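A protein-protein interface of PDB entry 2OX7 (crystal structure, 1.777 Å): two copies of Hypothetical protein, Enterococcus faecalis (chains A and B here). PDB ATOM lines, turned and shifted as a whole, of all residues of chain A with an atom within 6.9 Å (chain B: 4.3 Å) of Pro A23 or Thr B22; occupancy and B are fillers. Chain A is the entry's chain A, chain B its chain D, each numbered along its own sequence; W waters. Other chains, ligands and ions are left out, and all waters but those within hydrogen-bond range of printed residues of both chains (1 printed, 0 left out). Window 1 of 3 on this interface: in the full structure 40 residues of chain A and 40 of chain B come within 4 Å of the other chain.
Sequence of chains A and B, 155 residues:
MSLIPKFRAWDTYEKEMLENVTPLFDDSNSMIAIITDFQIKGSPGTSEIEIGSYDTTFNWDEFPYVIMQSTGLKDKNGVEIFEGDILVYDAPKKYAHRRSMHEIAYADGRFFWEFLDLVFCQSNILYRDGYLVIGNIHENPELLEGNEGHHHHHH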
ATOM      1  N   LYS A   6      17.101 -12.652  19.537  1.00  0.00           N
ATOM      2  CA  LYS A   6      15.831 -13.291  19.500  1.00  0.00           C
ATOM      3  C   LYS A   6      15.281 -13.174  20.906  1.00  0.00           C
ATOM      4  O   LYS A   6      16.008 -13.437  21.885  1.00  0.00           O
ATOM      5  CB  LYS A   6      15.980 -14.745  19.057  1.00  0.00           C
ATOM      6  CG  LYS A   6      14.691 -15.493  19.006  1.00  0.00           C
ATOM      7  CD  LYS A   6      14.920 -16.845  18.346  1.00  0.00           C
ATOM      8  CE  LYS A   6      13.624 -17.373  17.778  1.00  0.00           C
ATOM      9  NZ  LYS A   6      13.405 -16.752  16.421  1.00  0.00           N
ATOM     10  N   PHE A   7      14.015 -12.755  21.016  1.00  0.00           N
ATOM     11  CA  PHE A   7      13.431 -12.474  22.315  1.00  0.00           C
ATOM     12  C   PHE A   7      12.104 -13.167  22.512  1.00  0.00           C
ATOM     13  O   PHE A   7      11.339 -13.344  21.554  1.00  0.00           O
ATOM     14  CB  PHE A   7      13.207 -10.947  22.523  1.00  0.00           C
ATOM     15  CG  PHE A   7      14.466 -10.148  22.397  1.00  0.00           C
ATOM     16  CD1 PHE A   7      15.346 -10.026  23.474  1.00  0.00           C
ATOM     17  CD2 PHE A   7      14.785  -9.546  21.192  1.00  0.00           C
ATOM     18  CE1 PHE A   7      16.543  -9.297  23.332  1.00  0.00           C
ATOM     19  CE2 PHE A   7      15.961  -8.840  21.038  1.00  0.00           C
ATOM     20  CZ  PHE A   7      16.842  -8.713  22.115  1.00  0.00           C
ATOM     21  N   VAL A  21       9.185 -12.008  19.912  1.00  0.00           N
ATOM     22  CA  VAL A  21       8.733 -10.604  20.046  1.00  0.00           C
ATOM     23  C   VAL A  21       9.859  -9.613  19.745  1.00  0.00           C
ATOM     24  O   VAL A  21      11.046  -9.968  19.820  1.00  0.00           O
ATOM     25  CB  VAL A  21       8.170 -10.287  21.470  1.00  0.00           C
ATOM     26  CG1 VAL A  21       7.076 -11.283  21.892  1.00  0.00           C
ATOM     27  CG2 VAL A  21       9.278 -10.211  22.555  1.00  0.00           C
ATOM     28  N   THR A  22       9.491  -8.367  19.423  1.00  0.00           N
ATOM     29  CA  THR A  22      10.480  -7.301  19.272  1.00  0.00           C
ATOM     30  C   THR A  22      10.253  -6.261  20.351  1.00  0.00           C
ATOM     31  O   THR A  22       9.251  -5.551  20.325  1.00  0.00           O
ATOM     32  CB  THR A  22      10.394  -6.640  17.878  1.00  0.00           C
ATOM     33  OG1 THR A  22      10.529  -7.650  16.871  1.00  0.00           O
ATOM     34  CG2 THR A  22      11.504  -5.610  17.691  1.00  0.00           C
ATOM     35  N   PRO A  23      11.162  -6.177  21.335  1.00  0.00           N
ATOM     36  CA  PRO A  23      10.986  -5.220  22.421  1.00  0.00           C
ATOM     37  C   PRO A  23      11.431  -3.821  21.997  1.00  0.00           C
ATOM     38  O   PRO A  23      12.423  -3.676  21.277  1.00  0.00           O
ATOM     39  CB  PRO A  23      11.902  -5.778  23.520  1.00  0.00           C
ATOM     40  CG  PRO A  23      13.003  -6.448  22.775  1.00  0.00           C
ATOM     41  CD  PRO A  23      12.407  -6.965  21.492  1.00  0.00           C
ATOM     42  N   LEU A  24      10.670  -2.796  22.395  1.00  0.00           N
ATOM     43  CA  LEU A  24      11.007  -1.423  22.002  1.00  0.00           C
ATOM     44  C   LEU A  24      11.352  -0.598  23.237  1.00  0.00           C
ATOM     45  O   LEU A  24      10.569  -0.534  24.182  1.00  0.00           O
ATOM     46  CB  LEU A  24       9.855  -0.770  21.198  1.00  0.00           C
ATOM     47  CG  LEU A  24       9.683  -1.086  19.700  1.00  0.00           C
ATOM     48  CD1 LEU A  24       9.570  -2.561  19.399  1.00  0.00           C
ATOM     49  CD2 LEU A  24       8.432  -0.377  19.138  1.00  0.00           C
ATOM     50  N   PHE A  25      12.536   0.008  23.231  1.00  0.00           N
ATOM     51  CA  PHE A  25      13.022   0.763  24.386  1.00  0.00           C
ATOM     52  C   PHE A  25      13.152   2.235  24.059  1.00  0.00           C
ATOM     53  O   PHE A  25      13.443   2.622  22.916  1.00  0.00           O
ATOM     54  CB  PHE A  25      14.387   0.239  24.854  1.00  0.00           C
ATOM     55  CG  PHE A  25      14.318  -1.114  25.474  1.00  0.00           C
ATOM     56  CD1 PHE A  25      14.325  -1.265  26.845  1.00  0.00           C
ATOM     57  CD2 PHE A  25      14.191  -2.244  24.675  1.00  0.00           C
ATOM     58  CE1 PHE A  25      14.233  -2.527  27.427  1.00  0.00           C
ATOM     59  CE2 PHE A  25      14.089  -3.502  25.253  1.00  0.00           C
ATOM     60  CZ  PHE A  25      14.100  -3.637  26.626  1.00  0.00           C
ATOM     61  N   MET A  31      11.669  -0.400  28.642  1.00  0.00           N
ATOM     62  CA  MET A  31      10.813  -0.942  27.597  1.00  0.00           C
ATOM     63  C   MET A  31       9.454  -0.257  27.651  1.00  0.00           C
ATOM     64  O   MET A  31       8.774  -0.283  28.686  1.00  0.00           O
ATOM     65  CB  MET A  31      10.633  -2.439  27.726  1.00  0.00           C
ATOM     66  CG  MET A  31       9.901  -3.036  26.558  1.00  0.00           C
ATOM     67  SD  MET A  31       9.653  -4.947  26.726  1.00  0.00           S
ATOM     68  CE  MET A  31       9.058  -5.072  28.584  1.00  0.00           C
ATOM     69  N   ILE A  32       9.087   0.364  26.536  1.00  0.00           N
ATOM     70  CA  ILE A  32       7.858   1.155  26.478  1.00  0.00           C
ATOM     71  C   ILE A  32       6.843   0.573  25.495  1.00  0.00           C
ATOM     72  O   ILE A  32       5.668   0.957  25.505  1.00  0.00           O
ATOM     73  CB  ILE A  32       8.140   2.661  26.225  1.00  0.00           C
ATOM     74  CG1 ILE A  32       8.873   2.881  24.889  1.00  0.00           C
ATOM     75  CG2 ILE A  32       8.902   3.267  27.422  1.00  0.00           C
ATOM     76  CD1 ILE A  32       8.919   4.365  24.419  1.00  0.00           C
ATOM     77  N   ALA A  33       7.287  -0.371  24.664  1.00  0.00           N
ATOM     78  CA  ALA A  33       6.386  -1.058  23.738  1.00  0.00           C
ATOM     79  C   ALA A  33       6.867  -2.460  23.429  1.00  0.00           C
ATOM     80  O   ALA A  33       8.030  -2.805  23.666  1.00  0.00           O
ATOM     81  CB  ALA A  33       6.220  -0.254  22.430  1.00  0.00           C
ATOM     82  N   ILE A  34       5.959  -3.255  22.885  1.00  0.00           N
ATOM     83  CA  ILE A  34       6.308  -4.559  22.376  1.00  0.00           C
ATOM     84  C   ILE A  34       5.545  -4.839  21.089  1.00  0.00           C
ATOM     85  O   ILE A  34       4.324  -4.641  21.014  1.00  0.00           O
ATOM     86  CB  ILE A  34       6.111  -5.660  23.465  1.00  0.00           C
ATOM     87  CG1 ILE A  34       6.702  -6.995  23.018  1.00  0.00           C
ATOM     88  CG2 ILE A  34       4.643  -5.784  23.906  1.00  0.00           C
ATOM     89  CD1 ILE A  34       6.855  -7.978  24.182  1.00  0.00           C
ATOM     90  N   ILE A  35       6.284  -5.248  20.070  1.00  0.00           N
ATOM     91  CA  ILE A  35       5.691  -5.763  18.842  1.00  0.00           C
ATOM     92  C   ILE A  35       5.703  -7.286  18.886  1.00  0.00           C
ATOM     93  O   ILE A  35       6.779  -7.904  18.975  1.00  0.00           O
ATOM     94  CB  ILE A  35       6.472  -5.276  17.606  1.00  0.00           C
ATOM     95  CG1 ILE A  35       6.417  -3.738  17.523  1.00  0.00           C
ATOM     96  CG2 ILE A  35       5.924  -5.938  16.344  1.00  0.00           C
ATOM     97  CD1 ILE A  35       7.236  -3.115  16.399  1.00  0.00           C
ATOM     98  N   ILE A  49       6.575  -0.882   7.496  1.00  0.00           N
ATOM     99  CA  ILE A  49       6.404  -1.851   8.557  1.00  0.00           C
ATOM    100  C   ILE A  49       4.960  -1.815   9.020  1.00  0.00           C
ATOM    101  O   ILE A  49       4.517  -0.821   9.585  1.00  0.00           O
ATOM    102  CB  ILE A  49       7.305  -1.528   9.774  1.00  0.00           C
ATOM    103  CG1 ILE A  49       8.781  -1.545   9.375  1.00  0.00           C
ATOM    104  CG2 ILE A  49       6.996  -2.490  10.944  1.00  0.00           C
ATOM    105  CD1 ILE A  49       9.715  -0.855  10.365  1.00  0.00           C
ATOM    106  N   ILE A  67      11.086  -9.405  29.422  1.00  0.00           N
ATOM    107  CA  ILE A  67      11.811  -9.856  28.217  1.00  0.00           C
ATOM    108  C   ILE A  67      12.970 -10.791  28.592  1.00  0.00           C
ATOM    109  O   ILE A  67      13.625 -10.591  29.643  1.00  0.00           O
ATOM    110  CB  ILE A  67      12.359  -8.671  27.397  1.00  0.00           C
ATOM    111  CG1 ILE A  67      11.221  -7.752  26.961  1.00  0.00           C
ATOM    112  CG2 ILE A  67      13.099  -9.146  26.133  1.00  0.00           C
ATOM    113  CD1 ILE A  67      10.350  -8.316  25.829  1.00  0.00           C
ATOM    114  N   ASN B  20      20.628   3.499  19.316  1.00  0.00           N
ATOM    115  CA  ASN B  20      19.294   3.180  19.809  1.00  0.00           C
ATOM    116  C   ASN B  20      18.374   2.741  18.669  1.00  0.00           C
ATOM    117  O   ASN B  20      17.268   3.299  18.483  1.00  0.00           O
ATOM    118  CB  ASN B  20      18.710   4.376  20.560  1.00  0.00           C
ATOM    119  CG  ASN B  20      19.478   4.704  21.838  1.00  0.00           C
ATOM    120  OD1 ASN B  20      19.641   3.853  22.718  1.00  0.00           O
ATOM    121  ND2 ASN B  20      19.929   5.945  21.955  1.00  0.00           N
ATOM    122  N   VAL B  21      18.853   1.781  17.874  1.00  0.00           N
ATOM    123  CA  VAL B  21      18.031   1.241  16.790  1.00  0.00           C
ATOM    124  C   VAL B  21      17.323  -0.037  17.259  1.00  0.00           C
ATOM    125  O   VAL B  21      17.757  -0.693  18.225  1.00  0.00           O
ATOM    126  CB  VAL B  21      18.827   0.930  15.514  1.00  0.00           C
ATOM    127  CG1 VAL B  21      19.748   2.090  15.099  1.00  0.00           C
ATOM    128  CG2 VAL B  21      19.635  -0.368  15.633  1.00  0.00           C
ATOM    129  N   THR B  22      16.238  -0.380  16.566  1.00  0.00           N
ATOM    130  CA  THR B  22      15.492  -1.600  16.846  1.00  0.00           C
ATOM    131  C   THR B  22      15.500  -2.451  15.582  1.00  0.00           C
ATOM    132  O   THR B  22      14.841  -2.090  14.588  1.00  0.00           O
ATOM    133  CB  THR B  22      14.041  -1.295  17.225  1.00  0.00           C
ATOM    134  OG1 THR B  22      14.034  -0.458  18.380  1.00  0.00           O
ATOM    135  CG2 THR B  22      13.287  -2.591  17.557  1.00  0.00           C
ATOM    136  N   PRO B  23      16.242  -3.578  15.605  1.00  0.00           N
ATOM    137  CA  PRO B  23      16.293  -4.433  14.442  1.00  0.00           C
ATOM    138  C   PRO B  23      15.078  -5.343  14.451  1.00  0.00           C
ATOM    139  O   PRO B  23      14.596  -5.736  15.521  1.00  0.00           O
ATOM    140  CB  PRO B  23      17.587  -5.237  14.663  1.00  0.00           C
ATOM    141  CG  PRO B  23      17.684  -5.350  16.118  1.00  0.00           C
ATOM    142  CD  PRO B  23      17.073  -4.115  16.707  1.00  0.00           C
ATOM    143  N   LEU B  24      14.567  -5.639  13.268  1.00  0.00           N
ATOM    144  CA  LEU B  24      13.375  -6.464  13.129  1.00  0.00           C
ATOM    145  C   LEU B  24      13.729  -7.657  12.262  1.00  0.00           C
ATOM    146  O   LEU B  24      14.253  -7.488  11.178  1.00  0.00           O
ATOM    147  CB  LEU B  24      12.243  -5.661  12.445  1.00  0.00           C
ATOM    148  CG  LEU B  24      11.559  -4.608  13.322  1.00  0.00           C
ATOM    149  CD1 LEU B  24      10.568  -3.826  12.447  1.00  0.00           C
ATOM    150  CD2 LEU B  24      10.799  -5.241  14.431  1.00  0.00           C
ATOM    151  N   ALA B  33      14.198  -5.351   8.591  1.00  0.00           N
ATOM    152  CA  ALA B  33      13.916  -3.923   8.787  1.00  0.00           C
ATOM    153  C   ALA B  33      14.564  -3.367  10.039  1.00  0.00           C
ATOM    154  O   ALA B  33      15.081  -4.102  10.915  1.00  0.00           O
ATOM    155  CB  ALA B  33      12.385  -3.671   8.819  1.00  0.00           C
ATOM    156  N   ILE B  34      14.532  -2.049  10.147  1.00  0.00           N
ATOM    157  CA  ILE B  34      15.121  -1.400  11.298  1.00  0.00           C
ATOM    158  C   ILE B  34      14.299  -0.157  11.609  1.00  0.00           C
ATOM    159  O   ILE B  34      13.864   0.550  10.682  1.00  0.00           O
ATOM    160  CB  ILE B  34      16.575  -1.055  10.995  1.00  0.00           C
ATOM    161  CG1 ILE B  34      17.303  -0.571  12.239  1.00  0.00           C
ATOM    162  CG2 ILE B  34      16.650   0.018   9.913  1.00  0.00           C
ATOM    163  CD1 ILE B  34      18.739  -0.189  11.952  1.00  0.00           C
ATOM    164  N   ILE B  35      14.013   0.055  12.892  1.00  0.00           N
ATOM    165  CA  ILE B  35      13.331   1.258  13.371  1.00  0.00           C
ATOM    166  C   ILE B  35      14.390   2.139  14.033  1.00  0.00           C
ATOM    167  O   ILE B  35      15.063   1.729  14.992  1.00  0.00           O
ATOM    168  CB  ILE B  35      12.192   0.953  14.378  1.00  0.00           C
ATOM    169  CG1 ILE B  35      11.059   0.165  13.712  1.00  0.00           C
ATOM    170  CG2 ILE B  35      11.581   2.243  14.945  1.00  0.00           C
ATOM    171  CD1 ILE B  35      10.038  -0.421  14.700  1.00  0.00           C
HETATM  172  O   HOH W   1      14.475  -0.555  21.116  1.00  0.00           O
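The backbone NH (N) of Thr A22 is in hydrogen-bond range of the backbone carbonyl oxygen (O) of Ile A35, at 2.8 Å.
The backbone carbonyl oxygen of Thr B22 is in hydrogen-bond range of the backbone NH of Ile B35, 2.9 Å away.
N of Leu B24 lies within hydrogen-bond range of O of Ala B33 (2.9 Å).
Thr A22 touches Thr B22 (CG2 to CG2, 3.5 Å).
Pro B23 touches Thr A22 (O to CG2, 3.8 Å).
Leu B24 touches Thr A22 (CD2 to CG2, 3.4 Å).
O of Pro A23 touches CG2 of Thr B22 (3.97 Å).
Leu B24 touches Ile A49 (CD1 to CD1, 3.7 Å).
Ile A49 touches Ile B35.
Pro A23 touches one residue of chain B.
Of chain A, only Thr A22 and Pro A23 come within 4 Å of Thr B22.
Printed residues of chain B within 4 Å of Ile A49: Leu B24 (3.7 Å) and Ile B35 (3.7 Å).
Printed residues of chain A within 4 Å of Ile B35: Ile A49 (3.7 Å).
The nearest printed residue of chain B that does not touch Pro A23 is Pro B23 (6.5 Å).
The nearest residue of chain A that does not touch Thr B22 is Leu A24 (4.1 Å).
The nearest printed residue of chain B that does not touch Ile A49 is Ala B33 (4.2 Å).
Of the 14 printed residues of chain A, 3 touch a printed residue of chain B.
Of the 8 printed residues of chain B, 4 touch a printed residue of chain A.
Printed residues of chain B that touch a printed residue of chain A: Thr B22, Pro B23, Leu B24 and Ile B35.
Hydrophobic or aromatic side chains of chain B that line the printed part of chain A: Leu B24 and Ile B35.
Thr B22 touches its own counterpart, Thr A22.
Thr A22 touches Pro B23, and with the chains exchanged Pro A23 touches Thr B22.
Thr A22 touches Leu B24, but with the chains exchanged Leu A24 does not touch Thr B22 (4.1 Å).
7 positions are printed for both chains.
Of the 6 pairs that touch across the chains among the printed residues, 3 have their exchanged pair printed and touching as well.
Water W1 lies within hydrogen-bond range of the side-chain hydroxyl (OG1) of Thr B22 (2.8 Å) and the backbone NH (N) of Phe A25 (2.9 Å).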
